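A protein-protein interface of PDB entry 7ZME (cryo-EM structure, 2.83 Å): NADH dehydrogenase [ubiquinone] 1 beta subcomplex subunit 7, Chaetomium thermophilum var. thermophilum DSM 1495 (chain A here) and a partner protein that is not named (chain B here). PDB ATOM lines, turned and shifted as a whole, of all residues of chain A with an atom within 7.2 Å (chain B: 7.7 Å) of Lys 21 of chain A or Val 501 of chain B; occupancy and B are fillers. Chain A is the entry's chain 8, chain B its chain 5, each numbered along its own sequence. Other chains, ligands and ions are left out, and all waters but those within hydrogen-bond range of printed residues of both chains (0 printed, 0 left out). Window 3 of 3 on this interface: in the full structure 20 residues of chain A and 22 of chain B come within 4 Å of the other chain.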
ATOM      1  N   GLU A  16       2.921  16.902 -25.472  1.00  0.00           N
ATOM      2  CA  GLU A  16       2.292  17.668 -24.359  1.00  0.00           C
ATOM      3  C   GLU A  16       2.367  19.160 -24.685  1.00  0.00           C
ATOM      4  O   GLU A  16       1.914  19.970 -23.855  1.00  0.00           O
ATOM      5  CB  GLU A  16       2.993  17.373 -23.031  1.00  0.00           C
ATOM      6  CG  GLU A  16       4.406  17.923 -22.952  1.00  0.00           C
ATOM      7  CD  GLU A  16       5.490  16.861 -22.909  1.00  0.00           C
ATOM      8  OE1 GLU A  16       6.665  17.227 -22.711  1.00  0.00           O
ATOM      9  OE2 GLU A  16       5.158  15.673 -23.079  1.00  0.00           O
ATOM     10  N   MET A  17       2.899  19.504 -25.857  1.00  0.00           N
ATOM     11  CA  MET A  17       3.069  20.896 -26.241  1.00  0.00           C
ATOM     12  C   MET A  17       2.108  21.317 -27.344  1.00  0.00           C
ATOM     13  O   MET A  17       1.818  22.512 -27.473  1.00  0.00           O
ATOM     14  CB  MET A  17       4.519  21.114 -26.675  1.00  0.00           C
ATOM     15  CG  MET A  17       4.930  22.505 -27.035  1.00  0.00           C
ATOM     16  SD  MET A  17       6.692  22.405 -27.387  1.00  0.00           S
ATOM     17  CE  MET A  17       7.035  24.066 -27.893  1.00  0.00           C
ATOM     18  N   ARG A  18       1.611  20.364 -28.133  1.00  0.00           N
ATOM     19  CA  ARG A  18       0.429  20.620 -28.947  1.00  0.00           C
ATOM     20  C   ARG A  18      -0.822  20.653 -28.079  1.00  0.00           C
ATOM     21  O   ARG A  18      -1.733  21.453 -28.318  1.00  0.00           O
ATOM     22  CB  ARG A  18       0.304  19.554 -30.036  1.00  0.00           C
ATOM     23  CG  ARG A  18      -1.006  19.589 -30.807  1.00  0.00           C
ATOM     24  CD  ARG A  18      -1.928  18.445 -30.401  1.00  0.00           C
ATOM     25  NE  ARG A  18      -1.219  17.175 -30.281  1.00  0.00           N
ATOM     26  CZ  ARG A  18      -0.952  16.369 -31.304  1.00  0.00           C
ATOM     27  NH1 ARG A  18      -0.302  15.231 -31.101  1.00  0.00           N
ATOM     28  NH2 ARG A  18      -1.336  16.699 -32.528  1.00  0.00           N
ATOM     29  N   ASP A  19      -0.877  19.790 -27.061  1.00  0.00           N
ATOM     30  CA  ASP A  19      -2.013  19.781 -26.145  1.00  0.00           C
ATOM     31  C   ASP A  19      -2.073  21.056 -25.314  1.00  0.00           C
ATOM     32  O   ASP A  19      -3.162  21.492 -24.929  1.00  0.00           O
ATOM     33  CB  ASP A  19      -1.938  18.559 -25.232  1.00  0.00           C
ATOM     34  CG  ASP A  19      -2.267  17.269 -25.959  1.00  0.00           C
ATOM     35  OD1 ASP A  19      -2.196  17.253 -27.207  1.00  0.00           O
ATOM     36  OD2 ASP A  19      -2.591  16.269 -25.285  1.00  0.00           O
ATOM     37  N   ALA A  20      -0.919  21.663 -25.025  1.00  0.00           N
ATOM     38  CA  ALA A  20      -0.897  22.902 -24.259  1.00  0.00           C
ATOM     39  C   ALA A  20      -1.401  24.091 -25.065  1.00  0.00           C
ATOM     40  O   ALA A  20      -1.704  25.134 -24.476  1.00  0.00           O
ATOM     41  CB  ALA A  20       0.516  23.181 -23.751  1.00  0.00           C
ATOM     42  N   LYS A  21      -1.491  23.955 -26.390  1.00  0.00           N
ATOM     43  CA  LYS A  21      -2.004  25.005 -27.271  1.00  0.00           C
ATOM     44  C   LYS A  21      -1.207  26.300 -27.130  1.00  0.00           C
ATOM     45  O   LYS A  21      -1.768  27.385 -26.966  1.00  0.00           O
ATOM     46  CB  LYS A  21      -3.494  25.255 -27.019  1.00  0.00           C
ATOM     47  CG  LYS A  21      -4.397  24.090 -27.380  1.00  0.00           C
ATOM     48  CD  LYS A  21      -5.855  24.428 -27.113  1.00  0.00           C
ATOM     49  CE  LYS A  21      -6.776  23.304 -27.555  1.00  0.00           C
ATOM     50  NZ  LYS A  21      -6.591  22.077 -26.732  1.00  0.00           N
ATOM     51  N   VAL A  22       0.115  26.185 -27.187  1.00  0.00           N
ATOM     52  CA  VAL A  22       0.964  27.373 -27.189  1.00  0.00           C
ATOM     53  C   VAL A  22       1.061  27.884 -28.623  1.00  0.00           C
ATOM     54  O   VAL A  22       0.877  27.105 -29.568  1.00  0.00           O
ATOM     55  CB  VAL A  22       2.345  27.084 -26.575  1.00  0.00           C
ATOM     56  CG1 VAL A  22       2.190  26.393 -25.229  1.00  0.00           C
ATOM     57  CG2 VAL A  22       3.200  26.259 -27.507  1.00  0.00           C
ATOM     58  N   PRO A  23       1.316  29.174 -28.835  1.00  0.00           N
ATOM     59  CA  PRO A  23       1.367  29.705 -30.203  1.00  0.00           C
ATOM     60  C   PRO A  23       2.518  29.121 -31.011  1.00  0.00           C
ATOM     61  O   PRO A  23       3.524  28.660 -30.470  1.00  0.00           O
ATOM     62  CB  PRO A  23       1.545  31.212 -29.986  1.00  0.00           C
ATOM     63  CG  PRO A  23       0.958  31.457 -28.626  1.00  0.00           C
ATOM     64  CD  PRO A  23       1.325  30.247 -27.827  1.00  0.00           C
ATOM     65  N   LEU A  24       2.348  29.142 -32.338  1.00  0.00           N
ATOM     66  CA  LEU A  24       3.327  28.525 -33.229  1.00  0.00           C
ATOM     67  C   LEU A  24       4.687  29.199 -33.113  1.00  0.00           C
ATOM     68  O   LEU A  24       5.722  28.528 -33.041  1.00  0.00           O
ATOM     69  CB  LEU A  24       2.858  28.584 -34.681  1.00  0.00           C
ATOM     70  CG  LEU A  24       1.889  27.549 -35.250  1.00  0.00           C
ATOM     71  CD1 LEU A  24       2.508  26.155 -35.233  1.00  0.00           C
ATOM     72  CD2 LEU A  24       0.551  27.583 -34.574  1.00  0.00           C
ATOM     73  N   ARG A  27       6.900  27.930 -30.318  1.00  0.00           N
ATOM     74  CA  ARG A  27       7.160  26.496 -30.232  1.00  0.00           C
ATOM     75  C   ARG A  27       8.666  26.265 -30.303  1.00  0.00           C
ATOM     76  O   ARG A  27       9.230  25.899 -31.338  1.00  0.00           O
ATOM     77  CB  ARG A  27       6.437  25.742 -31.339  1.00  0.00           C
ATOM     78  CG  ARG A  27       4.926  25.859 -31.334  1.00  0.00           C
ATOM     79  CD  ARG A  27       4.283  24.653 -30.689  1.00  0.00           C
ATOM     80  NE  ARG A  27       2.897  24.913 -30.326  1.00  0.00           N
ATOM     81  CZ  ARG A  27       1.849  24.460 -31.002  1.00  0.00           C
ATOM     82  NH1 ARG A  27       2.025  23.712 -32.082  1.00  0.00           N
ATOM     83  NH2 ARG A  27       0.623  24.752 -30.593  1.00  0.00           N
ATOM     84  N   ILE A  35       4.355  27.076 -20.769  1.00  0.00           N
ATOM     85  CA  ILE A  35       3.111  26.429 -20.346  1.00  0.00           C
ATOM     86  C   ILE A  35       2.676  26.871 -18.953  1.00  0.00           C
ATOM     87  O   ILE A  35       1.502  27.240 -18.787  1.00  0.00           O
ATOM     88  CB  ILE A  35       3.241  24.901 -20.471  1.00  0.00           C
ATOM     89  CG1 ILE A  35       3.486  24.504 -21.927  1.00  0.00           C
ATOM     90  CG2 ILE A  35       1.996  24.215 -19.937  1.00  0.00           C
ATOM     91  CD1 ILE A  35       3.860  23.051 -22.105  1.00  0.00           C
ATOM     92  N   ASN A  38       1.435  30.592 -19.081  1.00  0.00           N
ATOM     93  CA  ASN A  38       0.116  30.774 -19.659  1.00  0.00           C
ATOM     94  C   ASN A  38      -0.992  30.255 -18.760  1.00  0.00           C
ATOM     95  O   ASN A  38      -2.167  30.507 -19.049  1.00  0.00           O
ATOM     96  CB  ASN A  38       0.059  30.095 -21.021  1.00  0.00           C
ATOM     97  CG  ASN A  38       0.763  30.892 -22.095  1.00  0.00           C
ATOM     98  OD1 ASN A  38       1.324  31.951 -21.827  1.00  0.00           O
ATOM     99  ND2 ASN A  38       0.739  30.387 -23.317  1.00  0.00           N
ATOM    100  N   TYR A  46      -4.852  37.276 -16.438  1.00  0.00           N
ATOM    101  CA  TYR A  46      -3.810  38.007 -17.153  1.00  0.00           C
ATOM    102  C   TYR A  46      -3.382  39.281 -16.433  1.00  0.00           C
ATOM    103  O   TYR A  46      -2.763  40.157 -17.042  1.00  0.00           O
ATOM    104  CB  TYR A  46      -4.255  38.348 -18.580  1.00  0.00           C
ATOM    105  CG  TYR A  46      -4.340  37.170 -19.519  1.00  0.00           C
ATOM    106  CD1 TYR A  46      -5.352  36.236 -19.397  1.00  0.00           C
ATOM    107  CD2 TYR A  46      -3.420  37.005 -20.540  1.00  0.00           C
ATOM    108  CE1 TYR A  46      -5.437  35.161 -20.252  1.00  0.00           C
ATOM    109  CE2 TYR A  46      -3.499  35.937 -21.404  1.00  0.00           C
ATOM    110  CZ  TYR A  46      -4.509  35.017 -21.255  1.00  0.00           C
ATOM    111  OH  TYR A  46      -4.592  33.947 -22.112  1.00  0.00           O
ATOM    112  N   GLY B  51     -12.852  35.239 -24.362  1.00  0.00           N
ATOM    113  CA  GLY B  51     -11.430  35.480 -24.259  1.00  0.00           C
ATOM    114  C   GLY B  51     -10.743  34.777 -23.110  1.00  0.00           C
ATOM    115  O   GLY B  51      -9.808  34.001 -23.324  1.00  0.00           O
ATOM    116  N   ASN B  53     -11.572  32.387 -21.313  1.00  0.00           N
ATOM    117  CA  ASN B  53     -11.771  30.950 -21.259  1.00  0.00           C
ATOM    118  C   ASN B  53     -11.373  30.235 -22.539  1.00  0.00           C
ATOM    119  O   ASN B  53     -11.350  28.999 -22.549  1.00  0.00           O
ATOM    120  CB  ASN B  53     -13.236  30.630 -20.943  1.00  0.00           C
ATOM    121  CG  ASN B  53     -13.629  31.054 -19.551  1.00  0.00           C
ATOM    122  OD1 ASN B  53     -13.109  30.533 -18.572  1.00  0.00           O
ATOM    123  ND2 ASN B  53     -14.556  31.998 -19.455  1.00  0.00           N
ATOM    124  N   ASN B  54     -11.059  30.971 -23.605  1.00  0.00           N
ATOM    125  CA  ASN B  54     -10.728  30.384 -24.903  1.00  0.00           C
ATOM    126  C   ASN B  54     -11.860  29.491 -25.408  1.00  0.00           C
ATOM    127  O   ASN B  54     -11.629  28.410 -25.949  1.00  0.00           O
ATOM    128  CB  ASN B  54      -9.407  29.612 -24.843  1.00  0.00           C
ATOM    129  CG  ASN B  54      -8.860  29.281 -26.217  1.00  0.00           C
ATOM    130  OD1 ASN B  54      -9.050  30.032 -27.173  1.00  0.00           O
ATOM    131  ND2 ASN B  54      -8.190  28.140 -26.325  1.00  0.00           N
ATOM    132  N   PRO B  56     -14.618  29.986 -28.050  1.00  0.00           N
ATOM    133  CA  PRO B  56     -15.402  30.673 -29.075  1.00  0.00           C
ATOM    134  C   PRO B  56     -16.774  30.037 -29.223  1.00  0.00           C
ATOM    135  O   PRO B  56     -16.988  28.864 -28.912  1.00  0.00           O
ATOM    136  CB  PRO B  56     -14.564  30.498 -30.344  1.00  0.00           C
ATOM    137  CG  PRO B  56     -13.736  29.311 -30.094  1.00  0.00           C
ATOM    138  CD  PRO B  56     -13.488  29.238 -28.619  1.00  0.00           C
ATOM    139  N   SER B  80     -11.592  35.592 -29.979  1.00  0.00           N
ATOM    140  CA  SER B  80     -10.816  36.541 -29.190  1.00  0.00           C
ATOM    141  C   SER B  80     -10.739  37.905 -29.860  1.00  0.00           C
ATOM    142  O   SER B  80     -10.697  38.927 -29.170  1.00  0.00           O
ATOM    143  CB  SER B  80      -9.413  36.000 -28.925  1.00  0.00           C
ATOM    144  OG  SER B  80      -9.446  34.878 -28.064  1.00  0.00           O
ATOM    145  N   GLY B 496       4.431  35.797 -24.203  1.00  0.00           N
ATOM    146  CA  GLY B 496       4.007  34.507 -24.708  1.00  0.00           C
ATOM    147  C   GLY B 496       2.537  34.237 -24.469  1.00  0.00           C
ATOM    148  O   GLY B 496       2.125  33.079 -24.365  1.00  0.00           O
ATOM    149  N   SER B 497       1.740  35.299 -24.375  1.00  0.00           N
ATOM    150  CA  SER B 497       0.342  35.157 -23.994  1.00  0.00           C
ATOM    151  C   SER B 497      -0.424  34.337 -25.025  1.00  0.00           C
ATOM    152  O   SER B 497      -0.100  34.332 -26.215  1.00  0.00           O
ATOM    153  CB  SER B 497      -0.303  36.532 -23.826  1.00  0.00           C
ATOM    154  OG  SER B 497      -0.575  37.129 -25.079  1.00  0.00           O
ATOM    155  N   ASN B 498      -1.450  33.634 -24.554  1.00  0.00           N
ATOM    156  CA  ASN B 498      -2.216  32.708 -25.374  1.00  0.00           C
ATOM    157  C   ASN B 498      -3.661  33.164 -25.516  1.00  0.00           C
ATOM    158  O   ASN B 498      -4.589  32.354 -25.521  1.00  0.00           O
ATOM    159  CB  ASN B 498      -2.180  31.296 -24.796  1.00  0.00           C
ATOM    160  CG  ASN B 498      -2.504  31.261 -23.320  1.00  0.00           C
ATOM    161  OD1 ASN B 498      -2.786  32.291 -22.709  1.00  0.00           O
ATOM    162  ND2 ASN B 498      -2.521  30.064 -22.750  1.00  0.00           N
ATOM    163  N   PHE B 499      -3.879  34.473 -25.617  1.00  0.00           N
ATOM    164  CA  PHE B 499      -5.247  34.969 -25.693  1.00  0.00           C
ATOM    165  C   PHE B 499      -5.891  34.633 -27.030  1.00  0.00           C
ATOM    166  O   PHE B 499      -7.054  34.215 -27.078  1.00  0.00           O
ATOM    167  CB  PHE B 499      -5.270  36.475 -25.450  1.00  0.00           C
ATOM    168  CG  PHE B 499      -6.604  36.994 -25.023  1.00  0.00           C
ATOM    169  CD1 PHE B 499      -7.071  36.761 -23.744  1.00  0.00           C
ATOM    170  CD2 PHE B 499      -7.394  37.716 -25.902  1.00  0.00           C
ATOM    171  CE1 PHE B 499      -8.299  37.237 -23.350  1.00  0.00           C
ATOM    172  CE2 PHE B 499      -8.622  38.194 -25.510  1.00  0.00           C
ATOM    173  CZ  PHE B 499      -9.075  37.958 -24.235  1.00  0.00           C
ATOM    174  N   PHE B 500      -5.168  34.831 -28.126  1.00  0.00           N
ATOM    175  CA  PHE B 500      -5.694  34.577 -29.467  1.00  0.00           C
ATOM    176  C   PHE B 500      -5.234  33.220 -29.995  1.00  0.00           C
ATOM    177  O   PHE B 500      -4.620  33.113 -31.056  1.00  0.00           O
ATOM    178  CB  PHE B 500      -5.296  35.713 -30.401  1.00  0.00           C
ATOM    179  CG  PHE B 500      -5.441  37.068 -29.779  1.00  0.00           C
ATOM    180  CD1 PHE B 500      -4.396  37.641 -29.077  1.00  0.00           C
ATOM    181  CD2 PHE B 500      -6.634  37.754 -29.870  1.00  0.00           C
ATOM    182  CE1 PHE B 500      -4.538  38.878 -28.489  1.00  0.00           C
ATOM    183  CE2 PHE B 500      -6.781  38.990 -29.283  1.00  0.00           C
ATOM    184  CZ  PHE B 500      -5.729  39.554 -28.591  1.00  0.00           C
ATOM    185  N   VAL B 501      -5.553  32.162 -29.249  1.00  0.00           N
ATOM    186  CA  VAL B 501      -5.177  30.806 -29.636  1.00  0.00           C
ATOM    187  C   VAL B 501      -6.323  30.045 -30.288  1.00  0.00           C
ATOM    188  O   VAL B 501      -6.258  28.820 -30.409  1.00  0.00           O
ATOM    189  CB  VAL B 501      -4.605  30.016 -28.453  1.00  0.00           C
ATOM    190  CG1 VAL B 501      -3.356  30.671 -27.968  1.00  0.00           C
ATOM    191  CG2 VAL B 501      -5.626  29.922 -27.338  1.00  0.00           C
ATOM    192  N   ASP B 502      -7.378  30.740 -30.706  1.00  0.00           N
ATOM    193  CA  ASP B 502      -8.374  30.165 -31.596  1.00  0.00           C
ATOM    194  C   ASP B 502      -8.084  30.484 -33.055  1.00  0.00           C
ATOM    195  O   ASP B 502      -9.007  30.506 -33.880  1.00  0.00           O
ATOM    196  CB  ASP B 502      -9.768  30.640 -31.190  1.00  0.00           C
ATOM    197  CG  ASP B 502      -9.837  32.137 -30.983  1.00  0.00           C
ATOM    198  OD1 ASP B 502      -8.787  32.803 -31.075  1.00  0.00           O
ATOM    199  OD2 ASP B 502     -10.938  32.644 -30.703  1.00  0.00           O
ATOM    200  N   ASN B 503      -6.814  30.714 -33.387  1.00  0.00           N
ATOM    201  CA  ASN B 503      -6.403  31.204 -34.700  1.00  0.00           C
ATOM    202  C   ASN B 503      -7.170  32.467 -35.066  1.00  0.00           C
ATOM    203  O   ASN B 503      -7.634  32.640 -36.194  1.00  0.00           O
ATOM    204  CB  ASN B 503      -6.565  30.140 -35.783  1.00  0.00           C
ATOM    205  CG  ASN B 503      -5.815  30.493 -37.048  1.00  0.00           C
ATOM    206  OD1 ASN B 503      -4.976  31.389 -37.050  1.00  0.00           O
ATOM    207  ND2 ASN B 503      -6.140  29.821 -38.138  1.00  0.00           N
ATOM    208  N   SER B 504      -7.317  33.357 -34.092  1.00  0.00           N
ATOM    209  CA  SER B 504      -7.976  34.626 -34.356  1.00  0.00           C
ATOM    210  C   SER B 504      -6.997  35.624 -34.958  1.00  0.00           C
ATOM    211  O   SER B 504      -7.245  36.180 -36.033  1.00  0.00           O
ATOM    212  CB  SER B 504      -8.584  35.167 -33.069  1.00  0.00           C
ATOM    213  OG  SER B 504      -9.471  36.220 -33.349  1.00  0.00           O
ATOM    214  N   LEU B 505      -5.881  35.855 -34.279  1.00  0.00           N
ATOM    215  CA  LEU B 505      -4.778  36.648 -34.800  1.00  0.00           C
ATOM    216  C   LEU B 505      -3.628  35.687 -35.071  1.00  0.00           C
ATOM    217  O   LEU B 505      -3.029  35.150 -34.134  1.00  0.00           O
ATOM    218  CB  LEU B 505      -4.373  37.741 -33.813  1.00  0.00           C
ATOM    219  CG  LEU B 505      -5.358  38.899 -33.659  1.00  0.00           C
ATOM    220  CD1 LEU B 505      -4.872  39.881 -32.611  1.00  0.00           C
ATOM    221  CD2 LEU B 505      -5.598  39.594 -34.984  1.00  0.00           C
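The side-chain amide nitrogen of Asn 498 of chain B lies close to the side-chain amide nitrogen of Asn 38 of chain A. OD1 of Asn 38 of chain A lies close to O of Gly 496 of chain B, at 2.9 Å. OD1 of Asn 498 of chain B lies within hydrogen-bond range of OH of Tyr 46 of chain A (2.5 Å).
The side-chain hydroxyl of Ser 80 of chain B lies within hydrogen-bond range of the backbone carbonyl oxygen of Phe 499 of chain B (2.7 Å).
Among the printed residues, merely in contact across the chains: Tyr 46 of chain A with Phe 499 of chain B, Lys 21 of chain A with Val 501 of chain B, Pro 23 of chain A with Ser 497 of chain B and Asn 38 of chain A with Ser 497 of chain B.
Of chain B, only Val 501 comes within 4 Å of Lys 21 of chain A. Of the printed residues of chain B, Pro 23 of chain A touches Ser 497. Of the printed residues of chain B, Asn 38 of chain A touches Gly 496, Ser 497 and Asn 498. Printed residues of chain B within 4 Å of Tyr 46 of chain A: Asn 498 and Phe 499. Asn 54 of chain B touches none of the printed residues of chain A. Of the printed residues of chain A, Phe 499 of chain B touches Tyr 46 (3.6 Å). Ser 504 of chain B touches none of the printed residues of chain A.
Of the 15 printed residues of chain B, 5 touch a printed residue of chain A. Hydrophobic or aromatic side chains of chain B that line the printed part of chain A: Phe 499 and Val 501. Among the printed residues, 7 pairs touch across the chains. Among the printed residues, no Asp or Glu carboxylate lies within 4 Å of a Lys or Arg side-chain nitrogen of the other chain.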
